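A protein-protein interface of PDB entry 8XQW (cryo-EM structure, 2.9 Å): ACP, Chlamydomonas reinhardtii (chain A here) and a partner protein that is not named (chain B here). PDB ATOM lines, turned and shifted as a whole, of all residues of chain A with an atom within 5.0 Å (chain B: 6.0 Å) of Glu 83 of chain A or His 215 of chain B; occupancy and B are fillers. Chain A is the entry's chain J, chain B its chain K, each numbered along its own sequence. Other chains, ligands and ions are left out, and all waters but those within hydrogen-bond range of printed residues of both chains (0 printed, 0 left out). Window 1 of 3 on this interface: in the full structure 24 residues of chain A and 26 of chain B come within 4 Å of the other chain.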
ATOM      1  N   MET A  79     -32.956  12.423  35.139  1.00  0.00           N
ATOM      2  CA  MET A  79     -31.535  12.727  34.987  1.00  0.00           C
ATOM      3  C   MET A  79     -31.325  14.083  34.330  1.00  0.00           C
ATOM      4  O   MET A  79     -30.445  14.854  34.734  1.00  0.00           O
ATOM      5  CB  MET A  79     -30.840  11.645  34.170  1.00  0.00           C
ATOM      6  CG  MET A  79     -30.850  10.287  34.809  1.00  0.00           C
ATOM      7  SD  MET A  79     -30.223  10.315  36.486  1.00  0.00           S
ATOM      8  CE  MET A  79     -31.560   9.507  37.352  1.00  0.00           C
ATOM      9  N   MET A  80     -32.124  14.395  33.315  1.00  0.00           N
ATOM     10  CA  MET A  80     -31.988  15.686  32.658  1.00  0.00           C
ATOM     11  C   MET A  80     -32.354  16.825  33.595  1.00  0.00           C
ATOM     12  O   MET A  80     -31.676  17.857  33.610  1.00  0.00           O
ATOM     13  CB  MET A  80     -32.836  15.726  31.397  1.00  0.00           C
ATOM     14  CG  MET A  80     -32.273  14.875  30.295  1.00  0.00           C
ATOM     15  SD  MET A  80     -33.398  14.662  28.916  1.00  0.00           S
ATOM     16  CE  MET A  80     -32.549  13.375  28.017  1.00  0.00           C
ATOM     17  N   ALA A  81     -33.409  16.663  34.391  1.00  0.00           N
ATOM     18  CA  ALA A  81     -33.755  17.697  35.355  1.00  0.00           C
ATOM     19  C   ALA A  81     -32.646  17.882  36.377  1.00  0.00           C
ATOM     20  O   ALA A  81     -32.350  19.010  36.786  1.00  0.00           O
ATOM     21  CB  ALA A  81     -35.064  17.354  36.055  1.00  0.00           C
ATOM     22  N   LEU A  82     -32.018  16.788  36.797  1.00  0.00           N
ATOM     23  CA  LEU A  82     -30.924  16.888  37.755  1.00  0.00           C
ATOM     24  C   LEU A  82     -29.773  17.691  37.182  1.00  0.00           C
ATOM     25  O   LEU A  82     -29.271  18.626  37.817  1.00  0.00           O
ATOM     26  CB  LEU A  82     -30.448  15.497  38.149  1.00  0.00           C
ATOM     27  CG  LEU A  82     -31.277  14.799  39.212  1.00  0.00           C
ATOM     28  CD1 LEU A  82     -30.637  13.483  39.583  1.00  0.00           C
ATOM     29  CD2 LEU A  82     -31.396  15.692  40.418  1.00  0.00           C
ATOM     30  N   GLU A  83     -29.330  17.330  35.980  1.00  0.00           N
ATOM     31  CA  GLU A  83     -28.244  18.065  35.345  1.00  0.00           C
ATOM     32  C   GLU A  83     -28.610  19.526  35.160  1.00  0.00           C
ATOM     33  O   GLU A  83     -27.781  20.417  35.360  1.00  0.00           O
ATOM     34  CB  GLU A  83     -27.906  17.440  34.002  1.00  0.00           C
ATOM     35  CG  GLU A  83     -27.404  16.040  34.095  1.00  0.00           C
ATOM     36  CD  GLU A  83     -26.933  15.538  32.763  1.00  0.00           C
ATOM     37  OE1 GLU A  83     -26.036  14.672  32.733  1.00  0.00           O
ATOM     38  OE2 GLU A  83     -27.454  16.021  31.738  1.00  0.00           O
ATOM     39  N   GLU A  84     -29.850  19.790  34.770  1.00  0.00           N
ATOM     40  CA  GLU A  84     -30.269  21.160  34.519  1.00  0.00           C
ATOM     41  C   GLU A  84     -30.262  21.980  35.800  1.00  0.00           C
ATOM     42  O   GLU A  84     -29.949  23.172  35.779  1.00  0.00           O
ATOM     43  CB  GLU A  84     -31.652  21.151  33.885  1.00  0.00           C
ATOM     44  CG  GLU A  84     -32.240  22.502  33.659  1.00  0.00           C
ATOM     45  CD  GLU A  84     -33.394  22.454  32.692  1.00  0.00           C
ATOM     46  OE1 GLU A  84     -33.748  23.514  32.131  1.00  0.00           O
ATOM     47  OE2 GLU A  84     -33.944  21.352  32.493  1.00  0.00           O
ATOM     48  N   LYS A  85     -30.600  21.360  36.926  1.00  0.00           N
ATOM     49  CA  LYS A  85     -30.593  22.099  38.182  1.00  0.00           C
ATOM     50  C   LYS A  85     -29.178  22.318  38.691  1.00  0.00           C
ATOM     51  O   LYS A  85     -28.852  23.407  39.164  1.00  0.00           O
ATOM     52  CB  LYS A  85     -31.427  21.370  39.229  1.00  0.00           C
ATOM     53  CG  LYS A  85     -30.976  21.615  40.651  1.00  0.00           C
ATOM     54  CD  LYS A  85     -31.366  23.000  41.130  1.00  0.00           C
ATOM     55  CE  LYS A  85     -30.967  23.204  42.578  1.00  0.00           C
ATOM     56  NZ  LYS A  85     -31.717  24.318  43.214  1.00  0.00           N
ATOM     57  N   PHE A  86     -28.325  21.306  38.612  1.00  0.00           N
ATOM     58  CA  PHE A  86     -26.992  21.436  39.183  1.00  0.00           C
ATOM     59  C   PHE A  86     -25.971  22.017  38.220  1.00  0.00           C
ATOM     60  O   PHE A  86     -24.873  22.366  38.658  1.00  0.00           O
ATOM     61  CB  PHE A  86     -26.503  20.085  39.687  1.00  0.00           C
ATOM     62  CG  PHE A  86     -27.038  19.724  41.028  1.00  0.00           C
ATOM     63  CD1 PHE A  86     -28.239  19.067  41.152  1.00  0.00           C
ATOM     64  CD2 PHE A  86     -26.350  20.055  42.168  1.00  0.00           C
ATOM     65  CE1 PHE A  86     -28.732  18.744  42.382  1.00  0.00           C
ATOM     66  CE2 PHE A  86     -26.845  19.732  43.397  1.00  0.00           C
ATOM     67  CZ  PHE A  86     -28.035  19.077  43.503  1.00  0.00           C
ATOM     68  N   GLU A  87     -26.302  22.127  36.934  1.00  0.00           N
ATOM     69  CA  GLU A  87     -25.435  22.714  35.913  1.00  0.00           C
ATOM     70  C   GLU A  87     -24.182  21.889  35.667  1.00  0.00           C
ATOM     71  O   GLU A  87     -23.145  22.432  35.297  1.00  0.00           O
ATOM     72  CB  GLU A  87     -25.043  24.147  36.266  1.00  0.00           C
ATOM     73  CG  GLU A  87     -26.147  25.155  36.068  1.00  0.00           C
ATOM     74  CD  GLU A  87     -25.659  26.579  36.210  1.00  0.00           C
ATOM     75  OE1 GLU A  87     -26.296  27.354  36.949  1.00  0.00           O
ATOM     76  OE2 GLU A  87     -24.639  26.925  35.583  1.00  0.00           O
ATOM     77  N   ILE A  88     -24.257  20.579  35.854  1.00  0.00           N
ATOM     78  CA  ILE A  88     -23.104  19.713  35.647  1.00  0.00           C
ATOM     79  C   ILE A  88     -23.399  18.734  34.526  1.00  0.00           C
ATOM     80  O   ILE A  88     -24.483  18.753  33.938  1.00  0.00           O
ATOM     81  CB  ILE A  88     -22.735  18.958  36.932  1.00  0.00           C
ATOM     82  CG1 ILE A  88     -23.933  18.149  37.413  1.00  0.00           C
ATOM     83  CG2 ILE A  88     -22.258  19.912  37.988  1.00  0.00           C
ATOM     84  CD1 ILE A  88     -23.627  16.704  37.666  1.00  0.00           C
ATOM     85  N   ALA A  89     -22.431  17.882  34.219  1.00  0.00           N
ATOM     86  CA  ALA A  89     -22.595  16.815  33.248  1.00  0.00           C
ATOM     87  C   ALA A  89     -22.331  15.484  33.928  1.00  0.00           C
ATOM     88  O   ALA A  89     -21.352  15.337  34.662  1.00  0.00           O
ATOM     89  CB  ALA A  89     -21.649  16.998  32.068  1.00  0.00           C
ATOM     90  N   LEU A  90     -23.202  14.514  33.680  1.00  0.00           N
ATOM     91  CA  LEU A  90     -23.116  13.222  34.342  1.00  0.00           C
ATOM     92  C   LEU A  90     -22.176  12.296  33.590  1.00  0.00           C
ATOM     93  O   LEU A  90     -22.095  12.336  32.360  1.00  0.00           O
ATOM     94  CB  LEU A  90     -24.496  12.574  34.441  1.00  0.00           C
ATOM     95  CG  LEU A  90     -25.446  13.125  35.496  1.00  0.00           C
ATOM     96  CD1 LEU A  90     -26.854  12.676  35.197  1.00  0.00           C
ATOM     97  CD2 LEU A  90     -25.023  12.663  36.872  1.00  0.00           C
ATOM     98  N   GLU A  92     -21.567   9.009  31.969  1.00  0.00           N
ATOM     99  CA  GLU A  92     -22.624   8.180  31.396  1.00  0.00           C
ATOM    100  C   GLU A  92     -22.512   6.719  31.812  1.00  0.00           C
ATOM    101  O   GLU A  92     -23.530   6.085  32.134  1.00  0.00           O
ATOM    102  CB  GLU A  92     -22.603   8.297  29.877  1.00  0.00           C
ATOM    103  CG  GLU A  92     -22.717   9.715  29.373  1.00  0.00           C
ATOM    104  CD  GLU A  92     -21.408  10.232  28.824  1.00  0.00           C
ATOM    105  OE1 GLU A  92     -21.326  11.433  28.497  1.00  0.00           O
ATOM    106  OE2 GLU A  92     -20.455   9.432  28.721  1.00  0.00           O
ATOM    107  N   THR B  94     -22.027  24.093  30.242  1.00  0.00           N
ATOM    108  CA  THR B  94     -22.433  22.706  30.170  1.00  0.00           C
ATOM    109  C   THR B  94     -22.196  22.187  28.760  1.00  0.00           C
ATOM    110  O   THR B  94     -21.853  22.940  27.849  1.00  0.00           O
ATOM    111  CB  THR B  94     -23.900  22.566  30.544  1.00  0.00           C
ATOM    112  OG1 THR B  94     -24.383  21.302  30.081  1.00  0.00           O
ATOM    113  CG2 THR B  94     -24.699  23.690  29.918  1.00  0.00           C
ATOM    114  N   GLY B  95     -22.372  20.886  28.583  1.00  0.00           N
ATOM    115  CA  GLY B  95     -22.179  20.363  27.248  1.00  0.00           C
ATOM    116  C   GLY B  95     -23.306  20.667  26.291  1.00  0.00           C
ATOM    117  O   GLY B  95     -23.095  20.611  25.077  1.00  0.00           O
ATOM    118  N   THR B  96     -24.475  21.008  26.801  1.00  0.00           N
ATOM    119  CA  THR B  96     -25.690  21.092  26.021  1.00  0.00           C
ATOM    120  C   THR B  96     -25.817  22.460  25.367  1.00  0.00           C
ATOM    121  O   THR B  96     -24.873  23.248  25.331  1.00  0.00           O
ATOM    122  CB  THR B  96     -26.882  20.785  26.913  1.00  0.00           C
ATOM    123  OG1 THR B  96     -26.911  21.718  27.994  1.00  0.00           O
ATOM    124  CG2 THR B  96     -26.757  19.408  27.487  1.00  0.00           C
ATOM    125  N   HIS B 179     -34.552  20.562  21.351  1.00  0.00           N
ATOM    126  CA  HIS B 179     -33.603  19.463  21.226  1.00  0.00           C
ATOM    127  C   HIS B 179     -33.868  18.376  22.256  1.00  0.00           C
ATOM    128  O   HIS B 179     -33.716  17.187  21.966  1.00  0.00           O
ATOM    129  CB  HIS B 179     -32.178  19.978  21.358  1.00  0.00           C
ATOM    130  CG  HIS B 179     -31.134  18.921  21.206  1.00  0.00           C
ATOM    131  ND1 HIS B 179     -30.841  18.332  19.997  1.00  0.00           N
ATOM    132  CD2 HIS B 179     -30.300  18.359  22.107  1.00  0.00           C
ATOM    133  CE1 HIS B 179     -29.879  17.446  20.164  1.00  0.00           C
ATOM    134  NE2 HIS B 179     -29.532  17.444  21.436  1.00  0.00           N
ATOM    135  N   ALA B 210     -28.676   8.019  25.453  1.00  0.00           N
ATOM    136  CA  ALA B 210     -29.481   9.227  25.588  1.00  0.00           C
ATOM    137  C   ALA B 210     -28.634  10.386  26.092  1.00  0.00           C
ATOM    138  O   ALA B 210     -28.650  11.483  25.517  1.00  0.00           O
ATOM    139  CB  ALA B 210     -30.650   8.972  26.530  1.00  0.00           C
ATOM    140  N   LEU B 211     -27.868  10.152  27.156  1.00  0.00           N
ATOM    141  CA  LEU B 211     -27.018  11.208  27.689  1.00  0.00           C
ATOM    142  C   LEU B 211     -25.925  11.606  26.711  1.00  0.00           C
ATOM    143  O   LEU B 211     -25.545  12.775  26.658  1.00  0.00           O
ATOM    144  CB  LEU B 211     -26.409  10.766  29.008  1.00  0.00           C
ATOM    145  CG  LEU B 211     -27.474  10.404  30.033  1.00  0.00           C
ATOM    146  CD1 LEU B 211     -26.850   9.706  31.204  1.00  0.00           C
ATOM    147  CD2 LEU B 211     -28.196  11.646  30.484  1.00  0.00           C
ATOM    148  N   ARG B 212     -25.403  10.661  25.933  1.00  0.00           N
ATOM    149  CA  ARG B 212     -24.392  11.020  24.954  1.00  0.00           C
ATOM    150  C   ARG B 212     -24.986  11.820  23.811  1.00  0.00           C
ATOM    151  O   ARG B 212     -24.306  12.664  23.228  1.00  0.00           O
ATOM    152  CB  ARG B 212     -23.704   9.768  24.433  1.00  0.00           C
ATOM    153  CG  ARG B 212     -22.620   9.287  25.355  1.00  0.00           C
ATOM    154  CD  ARG B 212     -22.104   7.952  24.941  1.00  0.00           C
ATOM    155  NE  ARG B 212     -21.965   7.872  23.501  1.00  0.00           N
ATOM    156  CZ  ARG B 212     -21.342   6.886  22.878  1.00  0.00           C
ATOM    157  NH1 ARG B 212     -20.800   5.905  23.577  1.00  0.00           N
ATOM    158  NH2 ARG B 212     -21.259   6.890  21.560  1.00  0.00           N
ATOM    159  N   ARG B 213     -26.247  11.571  23.480  1.00  0.00           N
ATOM    160  CA  ARG B 213     -26.912  12.359  22.453  1.00  0.00           C
ATOM    161  C   ARG B 213     -27.191  13.768  22.938  1.00  0.00           C
ATOM    162  O   ARG B 213     -27.181  14.715  22.149  1.00  0.00           O
ATOM    163  CB  ARG B 213     -28.207  11.676  22.041  1.00  0.00           C
ATOM    164  CG  ARG B 213     -28.059  10.760  20.871  1.00  0.00           C
ATOM    165  CD  ARG B 213     -29.399  10.410  20.299  1.00  0.00           C
ATOM    166  NE  ARG B 213     -29.974   9.260  20.976  1.00  0.00           N
ATOM    167  CZ  ARG B 213     -29.841   8.013  20.549  1.00  0.00           C
ATOM    168  NH1 ARG B 213     -29.157   7.764  19.446  1.00  0.00           N
ATOM    169  NH2 ARG B 213     -30.396   7.019  21.223  1.00  0.00           N
ATOM    170  N   LEU B 214     -27.465  13.928  24.228  1.00  0.00           N
ATOM    171  CA  LEU B 214     -27.788  15.257  24.725  1.00  0.00           C
ATOM    172  C   LEU B 214     -26.566  16.161  24.787  1.00  0.00           C
ATOM    173  O   LEU B 214     -26.699  17.382  24.695  1.00  0.00           O
ATOM    174  CB  LEU B 214     -28.438  15.158  26.097  1.00  0.00           C
ATOM    175  CG  LEU B 214     -29.198  16.407  26.515  1.00  0.00           C
ATOM    176  CD1 LEU B 214     -30.572  16.413  25.920  1.00  0.00           C
ATOM    177  CD2 LEU B 214     -29.265  16.479  28.012  1.00  0.00           C
ATOM    178  N   HIS B 215     -25.373  15.596  24.939  1.00  0.00           N
ATOM    179  CA  HIS B 215     -24.163  16.388  25.068  1.00  0.00           C
ATOM    180  C   HIS B 215     -23.355  16.437  23.783  1.00  0.00           C
ATOM    181  O   HIS B 215     -22.200  16.859  23.813  1.00  0.00           O
ATOM    182  CB  HIS B 215     -23.302  15.851  26.205  1.00  0.00           C
ATOM    183  CG  HIS B 215     -23.990  15.856  27.531  1.00  0.00           C
ATOM    184  ND1 HIS B 215     -24.458  17.007  28.120  1.00  0.00           N
ATOM    185  CD2 HIS B 215     -24.282  14.850  28.386  1.00  0.00           C
ATOM    186  CE1 HIS B 215     -25.016  16.712  29.279  1.00  0.00           C
ATOM    187  NE2 HIS B 215     -24.925  15.409  29.463  1.00  0.00           N
ATOM    188  N   TRP B 216     -23.932  16.013  22.662  1.00  0.00           N
ATOM    189  CA  TRP B 216     -23.294  16.094  21.349  1.00  0.00           C
ATOM    190  C   TRP B 216     -21.963  15.354  21.318  1.00  0.00           C
ATOM    191  O   TRP B 216     -20.941  15.899  20.911  1.00  0.00           O
ATOM    192  CB  TRP B 216     -23.100  17.544  20.927  1.00  0.00           C
ATOM    193  CG  TRP B 216     -24.349  18.300  20.810  1.00  0.00           C
ATOM    194  CD1 TRP B 216     -24.938  19.050  21.767  1.00  0.00           C
ATOM    195  CD2 TRP B 216     -25.172  18.402  19.655  1.00  0.00           C
ATOM    196  NE1 TRP B 216     -26.087  19.611  21.286  1.00  0.00           N
ATOM    197  CE2 TRP B 216     -26.251  19.225  19.985  1.00  0.00           C
ATOM    198  CE3 TRP B 216     -25.102  17.871  18.370  1.00  0.00           C
ATOM    199  CZ2 TRP B 216     -27.251  19.532  19.082  1.00  0.00           C
ATOM    200  CZ3 TRP B 216     -26.093  18.176  17.479  1.00  0.00           C
ATOM    201  CH2 TRP B 216     -27.152  18.999  17.835  1.00  0.00           C
ATOM    202  N   ARG B 217     -21.978  14.094  21.734  1.00  0.00           N
ATOM    203  CA  ARG B 217     -20.762  13.298  21.776  1.00  0.00           C
ATOM    204  C   ARG B 217     -20.754  12.177  20.754  1.00  0.00           C
ATOM    205  O   ARG B 217     -19.989  11.227  20.908  1.00  0.00           O
ATOM    206  CB  ARG B 217     -20.556  12.720  23.168  1.00  0.00           C
ATOM    207  CG  ARG B 217     -20.707  13.729  24.258  1.00  0.00           C
ATOM    208  CD  ARG B 217     -20.165  13.198  25.552  1.00  0.00           C
ATOM    209  NE  ARG B 217     -18.830  12.655  25.375  1.00  0.00           N
ATOM    210  CZ  ARG B 217     -17.742  13.396  25.231  1.00  0.00           C
ATOM    211  NH1 ARG B 217     -17.837  14.717  25.245  1.00  0.00           N
ATOM    212  NH2 ARG B 217     -16.561  12.820  25.073  1.00  0.00           N
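Of chain B, only His 215 (3.5 Å) comes within 4 Å of Glu 83 of chain A.
Of the printed residues of chain B, Glu 92 of chain A touches Leu 211, Arg 212 and Arg 217.
Of the printed residues of chain A, Leu 211 of chain B touches Glu 92 (3.9 Å).
Of the printed residues of chain A, Arg 212 of chain B touches Glu 92.
His 215 of chain B touches one residue of chain A.
Of the printed residues of chain A, Arg 217 of chain B touches Glu 92 (3.6 Å).
The nearest residue of chain A that does not touch His 215 of chain B is Ala 89 of chain A (4.4 Å).
The nearest printed residue of chain A that does not touch Arg 212 of chain B is Leu 90 of chain A (7.4 Å).
OE1 of Glu 83 of chain A is in hydrogen-bond range of N of Leu 90 of chain A (3.0 Å).
The backbone carbonyl oxygen (O) of Arg 212 of chain B is in hydrogen-bond range of the backbone NH (N) of Arg 217 of chain B, at 3.1 Å.
The side-chain carboxylate of Glu 83 of chain A sits at hydrogen-bond distance from a ring nitrogen (NE2) of His 215 of chain B.
Among the printed residues, pairs that only touch across the chains: Glu 92 of chain A with Leu 211 of chain B, Glu 92 of chain A with Arg 212 of chain B and Glu 92 of chain A with Arg 217 of chain B.
Printed residues of chain B that touch a printed residue of chain A: Leu 211, Arg 212, His 215 and Arg 217.
Along chain B the printed residues that touch a printed residue of chain A span positions 211 to 217.
Of the 13 printed residues of chain A, 2 touch a printed residue of chain B.
Among the printed residues, 4 pairs touch across the chains.
Among the printed residues, no Asp or Glu carboxylate lies within 4 Å of a Lys or Arg side-chain nitrogen of the other chain.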
